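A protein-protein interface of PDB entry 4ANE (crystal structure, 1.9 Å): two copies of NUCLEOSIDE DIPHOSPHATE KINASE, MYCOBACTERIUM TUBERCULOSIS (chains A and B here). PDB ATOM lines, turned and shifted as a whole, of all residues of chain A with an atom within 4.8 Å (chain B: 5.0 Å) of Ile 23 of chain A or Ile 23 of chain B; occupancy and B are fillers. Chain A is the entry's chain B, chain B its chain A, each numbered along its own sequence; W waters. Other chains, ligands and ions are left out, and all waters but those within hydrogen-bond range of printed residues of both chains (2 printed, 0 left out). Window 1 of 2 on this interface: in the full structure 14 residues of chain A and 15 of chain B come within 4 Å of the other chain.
The side-chain carboxylate (OE2) of Glu 21 of chain B lies within salt-bridge range of the guanidinium group (NE) of Arg 25 of chain B (2.8 Å).
The side-chain carboxylate of Glu 21 of chain A is in salt-bridge range of the guanidinium group of Arg 25 of chain A, at 2.7 Å.
OG of Ser 24 of chain B sits at hydrogen-bond distance from O of Gly 20 of chain B (3.0 Å).
The backbone carbonyl oxygen (O) of Gly 20 of chain A is in hydrogen-bond range of the side-chain hydroxyl (OG) of Ser 24 of chain A.
Ile 19 of chain A touches Glu 27 of chain B, and with the chains exchanged Glu 27 of chain A touches Ile 19 of chain B.
Gly 20 of chain A touches Glu 27 of chain B, and with the chains exchanged Glu 27 of chain A touches Gly 20 of chain B.
Glu 21 of chain A touches Ser 24 of chain B, and with the chains exchanged Ser 24 of chain A touches Glu 21 of chain B.
Ile 23 of chain B touches its own counterpart, Ile 23 of chain A.
Positions printed for both chains: 9, 19, 20, 21, 22, 23, 24, 25, 26, 27, 33 and 36.
Of the 16 pairs that touch across the chains among the printed residues, 15 have their exchanged pair printed and touching as well.
O of Gly 20 of chain B sits close to O of Gly 20 of chain A (3.4 Å).
The backbone NH (N) of Gly 20 of chain B sits at hydrogen-bond distance from the side-chain carboxylate (OE1) of Glu 27 of chain A, at 2.8 Å.
N of Glu 21 of chain B is in hydrogen-bond range of OG of Ser 24 of chain A.
The side-chain carboxylate (OE2) of Glu 27 of chain B is in hydrogen-bond range of the backbone NH (N) of Ile 19 of chain A.
OG of Ser 24 of chain B sits close to O of Gly 20 of chain A, at 3.5 Å.
The backbone NH (N) of Gly 20 of chain A sits at hydrogen-bond distance from the side-chain carboxylate (OE1) of Glu 27 of chain B, 2.8 Å away.
OE2 of Glu 27 of chain A lies within hydrogen-bond range of N of Leu 18 of chain B (3.4 Å).
OG of Ser 24 of chain B lies within hydrogen-bond range of N of Glu 21 of chain A (3.0 Å).
OE2 of Glu 27 of chain A is in hydrogen-bond range of N of Ile 19 of chain B (3.1 Å).
Of the 12 printed residues of chain A, 7 touch a printed residue of chain B.
Hydrophobic or aromatic side chains of chain A that line the printed part of chain B: Ile 19, Ile 23 and Leu 36.
Of the 13 printed residues of chain B, 8 touch a printed residue of chain A.
Printed residues of chain B that touch a printed residue of chain A: Leu 18, Ile 19, Gly 20, Glu 21, Ile 23, Ser 24, Glu 27 and Leu 36.
Hydrophobic or aromatic side chains of chain B that line the printed part of chain A: Ile 19, Ile 23 and Leu 36.
Among the printed residues, 16 pairs touch across the chains.
Water W2 lies within hydrogen-bond range of the side-chain carboxylate (OE1) of Glu 27 of chain B (2.7 Å), the backbone NH (N) of Glu 21 of chain A (2.9 Å), the backbone NH (N) of Gly 20 of chain A (3.2 Å) and the side-chain hydroxyl (OG) of Ser 24 of chain B (3.3 Å).
Water W1 lies within hydrogen-bond range of the side-chain carboxylate (OE1) of Glu 27 of chain A (2.7 Å), the backbone NH (N) of Glu 21 of chain B (2.9 Å), the side-chain hydroxyl (OG) of Ser 24 of chain A (3.2 Å) and the backbone NH (N) of Gly 20 of chain B (3.4 Å).
Of the printed residues of chain B, Ile 19 of chain A touches Ile 23 (3.9 Å) and Glu 27 (3.1 Å).
Of the printed residues of chain B, Ile 23 of chain A touches Ile 19 (3.95 Å), Gly 20 (3.6 Å) and Ile 23 (3.99 Å).
Ile 33 of chain A touches none of the printed residues of chain B.
Of the printed residues of chain A, Ile 23 of chain B touches Ile 19 (3.9 Å), Gly 20 (3.7 Å) and Ile 23 (3.99 Å).
Ile 33 of chain B touches none of the printed residues of chain A.
Of the printed residues of chain A, Leu 36 of chain B touches Leu 36.
The nearest printed residue of chain B that does not touch Ile 23 of chain A is Leu 36 of chain B (5.1 Å).
The nearest printed residue of chain A that does not touch Ile 23 of chain B is Leu 36 of chain A (4.8 Å).
Among the printed residues, merely in contact across the chains: Ser 24 of chain A with Gly 20 of chain B (3.0 Å), Ile 23 of chain A with Gly 20 of chain B (3.6 Å), Gly 20 of chain A with Ile 23 of chain B (3.7 Å), Ile 19 of chain A with Ile 23 of chain B (3.9 Å), Leu 36 of chain A with Leu 36 of chain B (3.9 Å), Ile 23 of chain A with Ile 19 of chain B (3.95 Å) and Ile 23 of chain A with Ile 23 of chain B (3.99 Å).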
ATOM      1  N   ILE A   9      32.547   4.262  22.341  1.00  0.00           N
ATOM      2  CA  ILE A   9      33.263   3.367  23.217  1.00  0.00           C
ATOM      3  C   ILE A   9      34.443   2.928  22.388  1.00  0.00           C
ATOM      4  O   ILE A   9      34.279   2.294  21.347  1.00  0.00           O
ATOM      5  CB  ILE A   9      32.413   2.172  23.650  1.00  0.00           C
ATOM      6  CG1 ILE A   9      31.179   2.671  24.397  1.00  0.00           C
ATOM      7  CG2 ILE A   9      33.248   1.220  24.537  1.00  0.00           C
ATOM      8  CD1 ILE A   9      30.228   1.583  24.854  1.00  0.00           C
ATOM      9  N   ILE A  19      31.303  -2.679  27.328  1.00  0.00           N
ATOM     10  CA  ILE A  19      30.202  -2.116  26.517  1.00  0.00           C
ATOM     11  C   ILE A  19      28.944  -1.943  27.350  1.00  0.00           C
ATOM     12  O   ILE A  19      28.354  -0.856  27.394  1.00  0.00           O
ATOM     13  CB  ILE A  19      29.857  -2.974  25.275  1.00  0.00           C
ATOM     14  CG1 ILE A  19      31.035  -3.037  24.315  1.00  0.00           C
ATOM     15  CG2 ILE A  19      28.634  -2.369  24.495  1.00  0.00           C
ATOM     16  CD1 ILE A  19      30.914  -4.147  23.272  1.00  0.00           C
ATOM     17  N   GLY A  20      28.534  -3.012  28.029  1.00  0.00           N
ATOM     18  CA  GLY A  20      27.295  -2.978  28.785  1.00  0.00           C
ATOM     19  C   GLY A  20      27.353  -2.019  29.961  1.00  0.00           C
ATOM     20  O   GLY A  20      26.408  -1.288  30.218  1.00  0.00           O
ATOM     21  N   GLU A  21      28.457  -2.047  30.698  1.00  0.00           N
ATOM     22  CA  GLU A  21      28.634  -1.134  31.827  1.00  0.00           C
ATOM     23  C   GLU A  21      28.451   0.332  31.421  1.00  0.00           C
ATOM     24  O   GLU A  21      27.767   1.125  32.095  1.00  0.00           O
ATOM     25  CB  GLU A  21      30.019  -1.336  32.453  1.00  0.00           C
ATOM     26  CG  GLU A  21      30.313  -0.357  33.590  1.00  0.00           C
ATOM     27  CD  GLU A  21      29.451  -0.626  34.806  1.00  0.00           C
ATOM     28  OE1 GLU A  21      29.159  -1.814  35.063  1.00  0.00           O
ATOM     29  OE2 GLU A  21      29.053   0.343  35.488  1.00  0.00           O
ATOM     30  N   ILE A  22      29.069   0.701  30.313  1.00  0.00           N
ATOM     31  CA  ILE A  22      29.050   2.086  29.874  1.00  0.00           C
ATOM     32  C   ILE A  22      27.653   2.497  29.422  1.00  0.00           C
ATOM     33  O   ILE A  22      27.189   3.582  29.757  1.00  0.00           O
ATOM     34  CB  ILE A  22      30.084   2.309  28.757  1.00  0.00           C
ATOM     35  CG1 ILE A  22      31.499   2.298  29.362  1.00  0.00           C
ATOM     36  CG2 ILE A  22      29.839   3.618  28.012  1.00  0.00           C
ATOM     37  CD1 ILE A  22      32.600   1.990  28.349  1.00  0.00           C
ATOM     38  N   ILE A  23      26.988   1.622  28.667  1.00  0.00           N
ATOM     39  CA  ILE A  23      25.607   1.884  28.244  1.00  0.00           C
ATOM     40  C   ILE A  23      24.657   1.965  29.446  1.00  0.00           C
ATOM     41  O   ILE A  23      23.811   2.865  29.501  1.00  0.00           O
ATOM     42  CB  ILE A  23      25.114   0.862  27.178  1.00  0.00           C
ATOM     43  CG1 ILE A  23      25.901   1.034  25.868  1.00  0.00           C
ATOM     44  CG2 ILE A  23      23.609   1.047  26.899  1.00  0.00           C
ATOM     45  CD1 ILE A  23      25.648  -0.078  24.845  1.00  0.00           C
ATOM     46  N   SER A  24      24.823   1.065  30.425  1.00  0.00           N
ATOM     47  CA  SER A  24      24.013   1.104  31.650  1.00  0.00           C
ATOM     48  C   SER A  24      24.111   2.448  32.373  1.00  0.00           C
ATOM     49  O   SER A  24      23.107   3.021  32.804  1.00  0.00           O
ATOM     50  CB  SER A  24      24.405  -0.015  32.634  1.00  0.00           C
ATOM     51  OG  SER A  24      24.002  -1.290  32.151  1.00  0.00           O
ATOM     52  N   ARG A  25      25.328   2.948  32.505  1.00  0.00           N
ATOM     53  CA  ARG A  25      25.526   4.227  33.175  1.00  0.00           C
ATOM     54  C   ARG A  25      24.806   5.351  32.460  1.00  0.00           C
ATOM     55  O   ARG A  25      24.237   6.231  33.104  1.00  0.00           O
ATOM     56  CB  ARG A  25      27.006   4.515  33.341  1.00  0.00           C
ATOM     57  CG  ARG A  25      27.587   3.617  34.440  1.00  0.00           C
ATOM     58  CD  ARG A  25      29.078   3.791  34.596  1.00  0.00           C
ATOM     59  NE  ARG A  25      29.590   2.968  35.698  1.00  0.00           N
ATOM     60  CZ  ARG A  25      30.371   3.437  36.661  1.00  0.00           C
ATOM     61  NH1 ARG A  25      30.708   4.716  36.651  1.00  0.00           N
ATOM     62  NH2 ARG A  25      30.817   2.635  37.619  1.00  0.00           N
ATOM     63  N   ILE A  26      24.804   5.304  31.132  1.00  0.00           N
ATOM     64  CA  ILE A  26      24.085   6.293  30.345  1.00  0.00           C
ATOM     65  C   ILE A  26      22.578   6.182  30.555  1.00  0.00           C
ATOM     66  O   ILE A  26      21.877   7.187  30.752  1.00  0.00           O
ATOM     67  CB  ILE A  26      24.461   6.201  28.842  1.00  0.00           C
ATOM     68  CG1 ILE A  26      25.912   6.663  28.640  1.00  0.00           C
ATOM     69  CG2 ILE A  26      23.503   7.040  27.996  1.00  0.00           C
ATOM     70  CD1 ILE A  26      26.539   6.187  27.333  1.00  0.00           C
ATOM     71  N   GLU A  27      22.080   4.950  30.531  1.00  0.00           N
ATOM     72  CA  GLU A  27      20.660   4.709  30.705  1.00  0.00           C
ATOM     73  C   GLU A  27      20.160   5.085  32.095  1.00  0.00           C
ATOM     74  O   GLU A  27      19.106   5.702  32.226  1.00  0.00           O
ATOM     75  CB  GLU A  27      20.326   3.239  30.394  1.00  0.00           C
ATOM     76  CG  GLU A  27      20.386   2.880  28.903  1.00  0.00           C
ATOM     77  CD  GLU A  27      20.145   1.389  28.679  1.00  0.00           C
ATOM     78  OE1 GLU A  27      20.955   0.591  29.202  1.00  0.00           O
ATOM     79  OE2 GLU A  27      19.135   1.015  28.019  1.00  0.00           O
ATOM     80  N   ILE A  33      19.241   5.818  24.314  1.00  0.00           N
ATOM     81  CA  ILE A  33      20.104   5.453  23.215  1.00  0.00           C
ATOM     82  C   ILE A  33      19.274   5.546  21.958  1.00  0.00           C
ATOM     83  O   ILE A  33      18.388   4.722  21.736  1.00  0.00           O
ATOM     84  CB  ILE A  33      20.585   4.015  23.378  1.00  0.00           C
ATOM     85  CG1 ILE A  33      21.219   3.828  24.763  1.00  0.00           C
ATOM     86  CG2 ILE A  33      21.521   3.638  22.235  1.00  0.00           C
ATOM     87  CD1 ILE A  33      22.427   4.735  25.012  1.00  0.00           C
ATOM     88  N   LEU A  36      22.842   3.096  17.721  1.00  0.00           N
ATOM     89  CA  LEU A  36      23.868   2.282  18.346  1.00  0.00           C
ATOM     90  C   LEU A  36      24.436   1.329  17.311  1.00  0.00           C
ATOM     91  O   LEU A  36      23.682   0.655  16.619  1.00  0.00           O
ATOM     92  CB  LEU A  36      23.259   1.496  19.522  1.00  0.00           C
ATOM     93  CG  LEU A  36      24.210   0.539  20.250  1.00  0.00           C
ATOM     94  CD1 LEU A  36      25.200   1.383  21.009  1.00  0.00           C
ATOM     95  CD2 LEU A  36      23.461  -0.380  21.202  1.00  0.00           C
ATOM     96  N   ILE B   9      17.441  -7.577  21.488  1.00  0.00           N
ATOM     97  CA  ILE B   9      16.794  -6.899  22.600  1.00  0.00           C
ATOM     98  C   ILE B   9      15.518  -6.313  22.029  1.00  0.00           C
ATOM     99  O   ILE B   9      15.573  -5.524  21.091  1.00  0.00           O
ATOM    100  CB  ILE B   9      17.693  -5.833  23.213  1.00  0.00           C
ATOM    101  CG1 ILE B   9      19.010  -6.488  23.662  1.00  0.00           C
ATOM    102  CG2 ILE B   9      16.993  -5.178  24.402  1.00  0.00           C
ATOM    103  CD1 ILE B   9      20.079  -5.500  24.171  1.00  0.00           C
ATOM    104  N   LEU B  18      17.188  -1.317  29.525  1.00  0.00           N
ATOM    105  CA  LEU B  18      17.911  -2.495  29.937  1.00  0.00           C
ATOM    106  C   LEU B  18      18.928  -2.919  28.877  1.00  0.00           C
ATOM    107  O   LEU B  18      19.473  -4.005  28.951  1.00  0.00           O
ATOM    108  CB  LEU B  18      16.941  -3.651  30.262  1.00  0.00           C
ATOM    109  CG  LEU B  18      16.245  -3.561  31.636  1.00  0.00           C
ATOM    110  CD1 LEU B  18      15.034  -4.485  31.729  1.00  0.00           C
ATOM    111  CD2 LEU B  18      17.223  -3.862  32.791  1.00  0.00           C
ATOM    112  N   ILE B  19      19.211  -2.058  27.904  1.00  0.00           N
ATOM    113  CA  ILE B  19      20.222  -2.412  26.896  1.00  0.00           C
ATOM    114  C   ILE B  19      21.569  -2.761  27.543  1.00  0.00           C
ATOM    115  O   ILE B  19      22.139  -3.816  27.274  1.00  0.00           O
ATOM    116  CB  ILE B  19      20.455  -1.284  25.877  1.00  0.00           C
ATOM    117  CG1 ILE B  19      19.152  -0.940  25.144  1.00  0.00           C
ATOM    118  CG2 ILE B  19      21.570  -1.678  24.885  1.00  0.00           C
ATOM    119  CD1 ILE B  19      19.256   0.303  24.254  1.00  0.00           C
ATOM    120  N   GLY B  20      22.078  -1.845  28.368  1.00  0.00           N
ATOM    121  CA  GLY B  20      23.350  -2.040  29.061  1.00  0.00           C
ATOM    122  C   GLY B  20      23.375  -3.255  29.971  1.00  0.00           C
ATOM    123  O   GLY B  20      24.343  -4.018  29.972  1.00  0.00           O
ATOM    124  N   GLU B  21      22.323  -3.424  30.769  1.00  0.00           N
ATOM    125  CA  GLU B  21      22.207  -4.568  31.665  1.00  0.00           C
ATOM    126  C   GLU B  21      22.325  -5.895  30.900  1.00  0.00           C
ATOM    127  O   GLU B  21      23.053  -6.807  31.304  1.00  0.00           O
ATOM    128  CB  GLU B  21      20.867  -4.523  32.403  1.00  0.00           C
ATOM    129  CG  GLU B  21      20.609  -5.722  33.326  1.00  0.00           C
ATOM    130  CD  GLU B  21      21.536  -5.743  34.548  1.00  0.00           C
ATOM    131  OE1 GLU B  21      21.845  -4.664  35.089  1.00  0.00           O
ATOM    132  OE2 GLU B  21      21.951  -6.841  34.963  1.00  0.00           O
ATOM    133  N   ILE B  22      21.611  -5.992  29.783  1.00  0.00           N
ATOM    134  CA  ILE B  22      21.611  -7.217  28.987  1.00  0.00           C
ATOM    135  C   ILE B  22      22.958  -7.473  28.339  1.00  0.00           C
ATOM    136  O   ILE B  22      23.457  -8.598  28.335  1.00  0.00           O
ATOM    137  CB  ILE B  22      20.480  -7.178  27.918  1.00  0.00           C
ATOM    138  CG1 ILE B  22      19.126  -7.277  28.634  1.00  0.00           C
ATOM    139  CG2 ILE B  22      20.681  -8.275  26.865  1.00  0.00           C
ATOM    140  CD1 ILE B  22      17.890  -6.861  27.809  1.00  0.00           C
ATOM    141  N   ILE B  23      23.560  -6.429  27.781  1.00  0.00           N
ATOM    142  CA  ILE B  23      24.841  -6.606  27.126  1.00  0.00           C
ATOM    143  C   ILE B  23      25.891  -6.964  28.192  1.00  0.00           C
ATOM    144  O   ILE B  23      26.735  -7.818  27.958  1.00  0.00           O
ATOM    145  CB  ILE B  23      25.252  -5.345  26.328  1.00  0.00           C
ATOM    146  CG1 ILE B  23      24.289  -5.142  25.143  1.00  0.00           C
ATOM    147  CG2 ILE B  23      26.701  -5.433  25.853  1.00  0.00           C
ATOM    148  CD1 ILE B  23      24.562  -3.884  24.343  1.00  0.00           C
ATOM    149  N   SER B  24      25.794  -6.340  29.366  1.00  0.00           N
ATOM    150  CA  SER B  24      26.719  -6.648  30.479  1.00  0.00           C
ATOM    151  C   SER B  24      26.687  -8.120  30.903  1.00  0.00           C
ATOM    152  O   SER B  24      27.730  -8.716  31.142  1.00  0.00           O
ATOM    153  CB  SER B  24      26.407  -5.794  31.712  1.00  0.00           C
ATOM    154  OG  SER B  24      26.889  -4.477  31.554  1.00  0.00           O
ATOM    155  N   ARG B  25      25.486  -8.678  31.034  1.00  0.00           N
ATOM    156  CA  ARG B  25      25.320 -10.088  31.393  1.00  0.00           C
ATOM    157  C   ARG B  25      25.981 -11.013  30.376  1.00  0.00           C
ATOM    158  O   ARG B  25      26.616 -11.994  30.746  1.00  0.00           O
ATOM    159  CB  ARG B  25      23.846 -10.433  31.586  1.00  0.00           C
ATOM    160  CG  ARG B  25      23.290  -9.826  32.881  1.00  0.00           C
ATOM    161  CD  ARG B  25      21.776  -9.896  33.007  1.00  0.00           C
ATOM    162  NE  ARG B  25      21.379  -9.469  34.354  1.00  0.00           N
ATOM    163  CZ  ARG B  25      20.694 -10.213  35.221  1.00  0.00           C
ATOM    164  NH1 ARG B  25      20.284 -11.437  34.896  1.00  0.00           N
ATOM    165  NH2 ARG B  25      20.389  -9.718  36.412  1.00  0.00           N
ATOM    166  N   ILE B  26      25.828 -10.690  29.098  1.00  0.00           N
ATOM    167  CA  ILE B  26      26.495 -11.417  28.023  1.00  0.00           C
ATOM    168  C   ILE B  26      28.018 -11.324  28.119  1.00  0.00           C
ATOM    169  O   ILE B  26      28.722 -12.335  28.029  1.00  0.00           O
ATOM    170  CB  ILE B  26      26.045 -10.905  26.648  1.00  0.00           C
ATOM    171  CG1 ILE B  26      24.554 -11.227  26.449  1.00  0.00           C
ATOM    172  CG2 ILE B  26      26.945 -11.505  25.539  1.00  0.00           C
ATOM    173  CD1 ILE B  26      23.883 -10.440  25.361  1.00  0.00           C
ATOM    174  N   GLU B  27      28.527 -10.108  28.306  1.00  0.00           N
ATOM    175  CA  GLU B  27      29.961  -9.921  28.430  1.00  0.00           C
ATOM    176  C   GLU B  27      30.548 -10.638  29.641  1.00  0.00           C
ATOM    177  O   GLU B  27      31.596 -11.267  29.527  1.00  0.00           O
ATOM    178  CB  GLU B  27      30.329  -8.436  28.464  1.00  0.00           C
ATOM    179  CG  GLU B  27      30.185  -7.712  27.107  1.00  0.00           C
ATOM    180  CD  GLU B  27      30.339  -6.206  27.246  1.00  0.00           C
ATOM    181  OE1 GLU B  27      29.539  -5.590  27.990  1.00  0.00           O
ATOM    182  OE2 GLU B  27      31.279  -5.653  26.641  1.00  0.00           O
ATOM    183  N   ILE B  33      30.729  -9.508  21.795  1.00  0.00           N
ATOM    184  CA  ILE B  33      29.768  -8.874  20.893  1.00  0.00           C
ATOM    185  C   ILE B  33      30.443  -8.691  19.531  1.00  0.00           C
ATOM    186  O   ILE B  33      31.320  -7.846  19.388  1.00  0.00           O
ATOM    187  CB  ILE B  33      29.337  -7.473  21.428  1.00  0.00           C
ATOM    188  CG1 ILE B  33      28.852  -7.560  22.874  1.00  0.00           C
ATOM    189  CG2 ILE B  33      28.269  -6.817  20.503  1.00  0.00           C
ATOM    190  CD1 ILE B  33      27.657  -8.483  23.073  1.00  0.00           C
ATOM    191  N   LEU B  36      26.498  -5.432  16.404  1.00  0.00           N
ATOM    192  CA  LEU B  36      25.557  -4.742  17.276  1.00  0.00           C
ATOM    193  C   LEU B  36      24.930  -3.583  16.517  1.00  0.00           C
ATOM    194  O   LEU B  36      25.639  -2.729  15.967  1.00  0.00           O
ATOM    195  CB  LEU B  36      26.283  -4.209  18.514  1.00  0.00           C
ATOM    196  CG  LEU B  36      25.472  -3.537  19.627  1.00  0.00           C
ATOM    197  CD1 LEU B  36      24.588  -4.554  20.334  1.00  0.00           C
ATOM    198  CD2 LEU B  36      26.412  -2.861  20.627  1.00  0.00           C
HETATM  199  O   HOH W   1      20.877  -0.948  31.406  1.00  0.00           O
HETATM  200  O   HOH W   2      29.936  -4.542  30.415  1.00  0.00           O
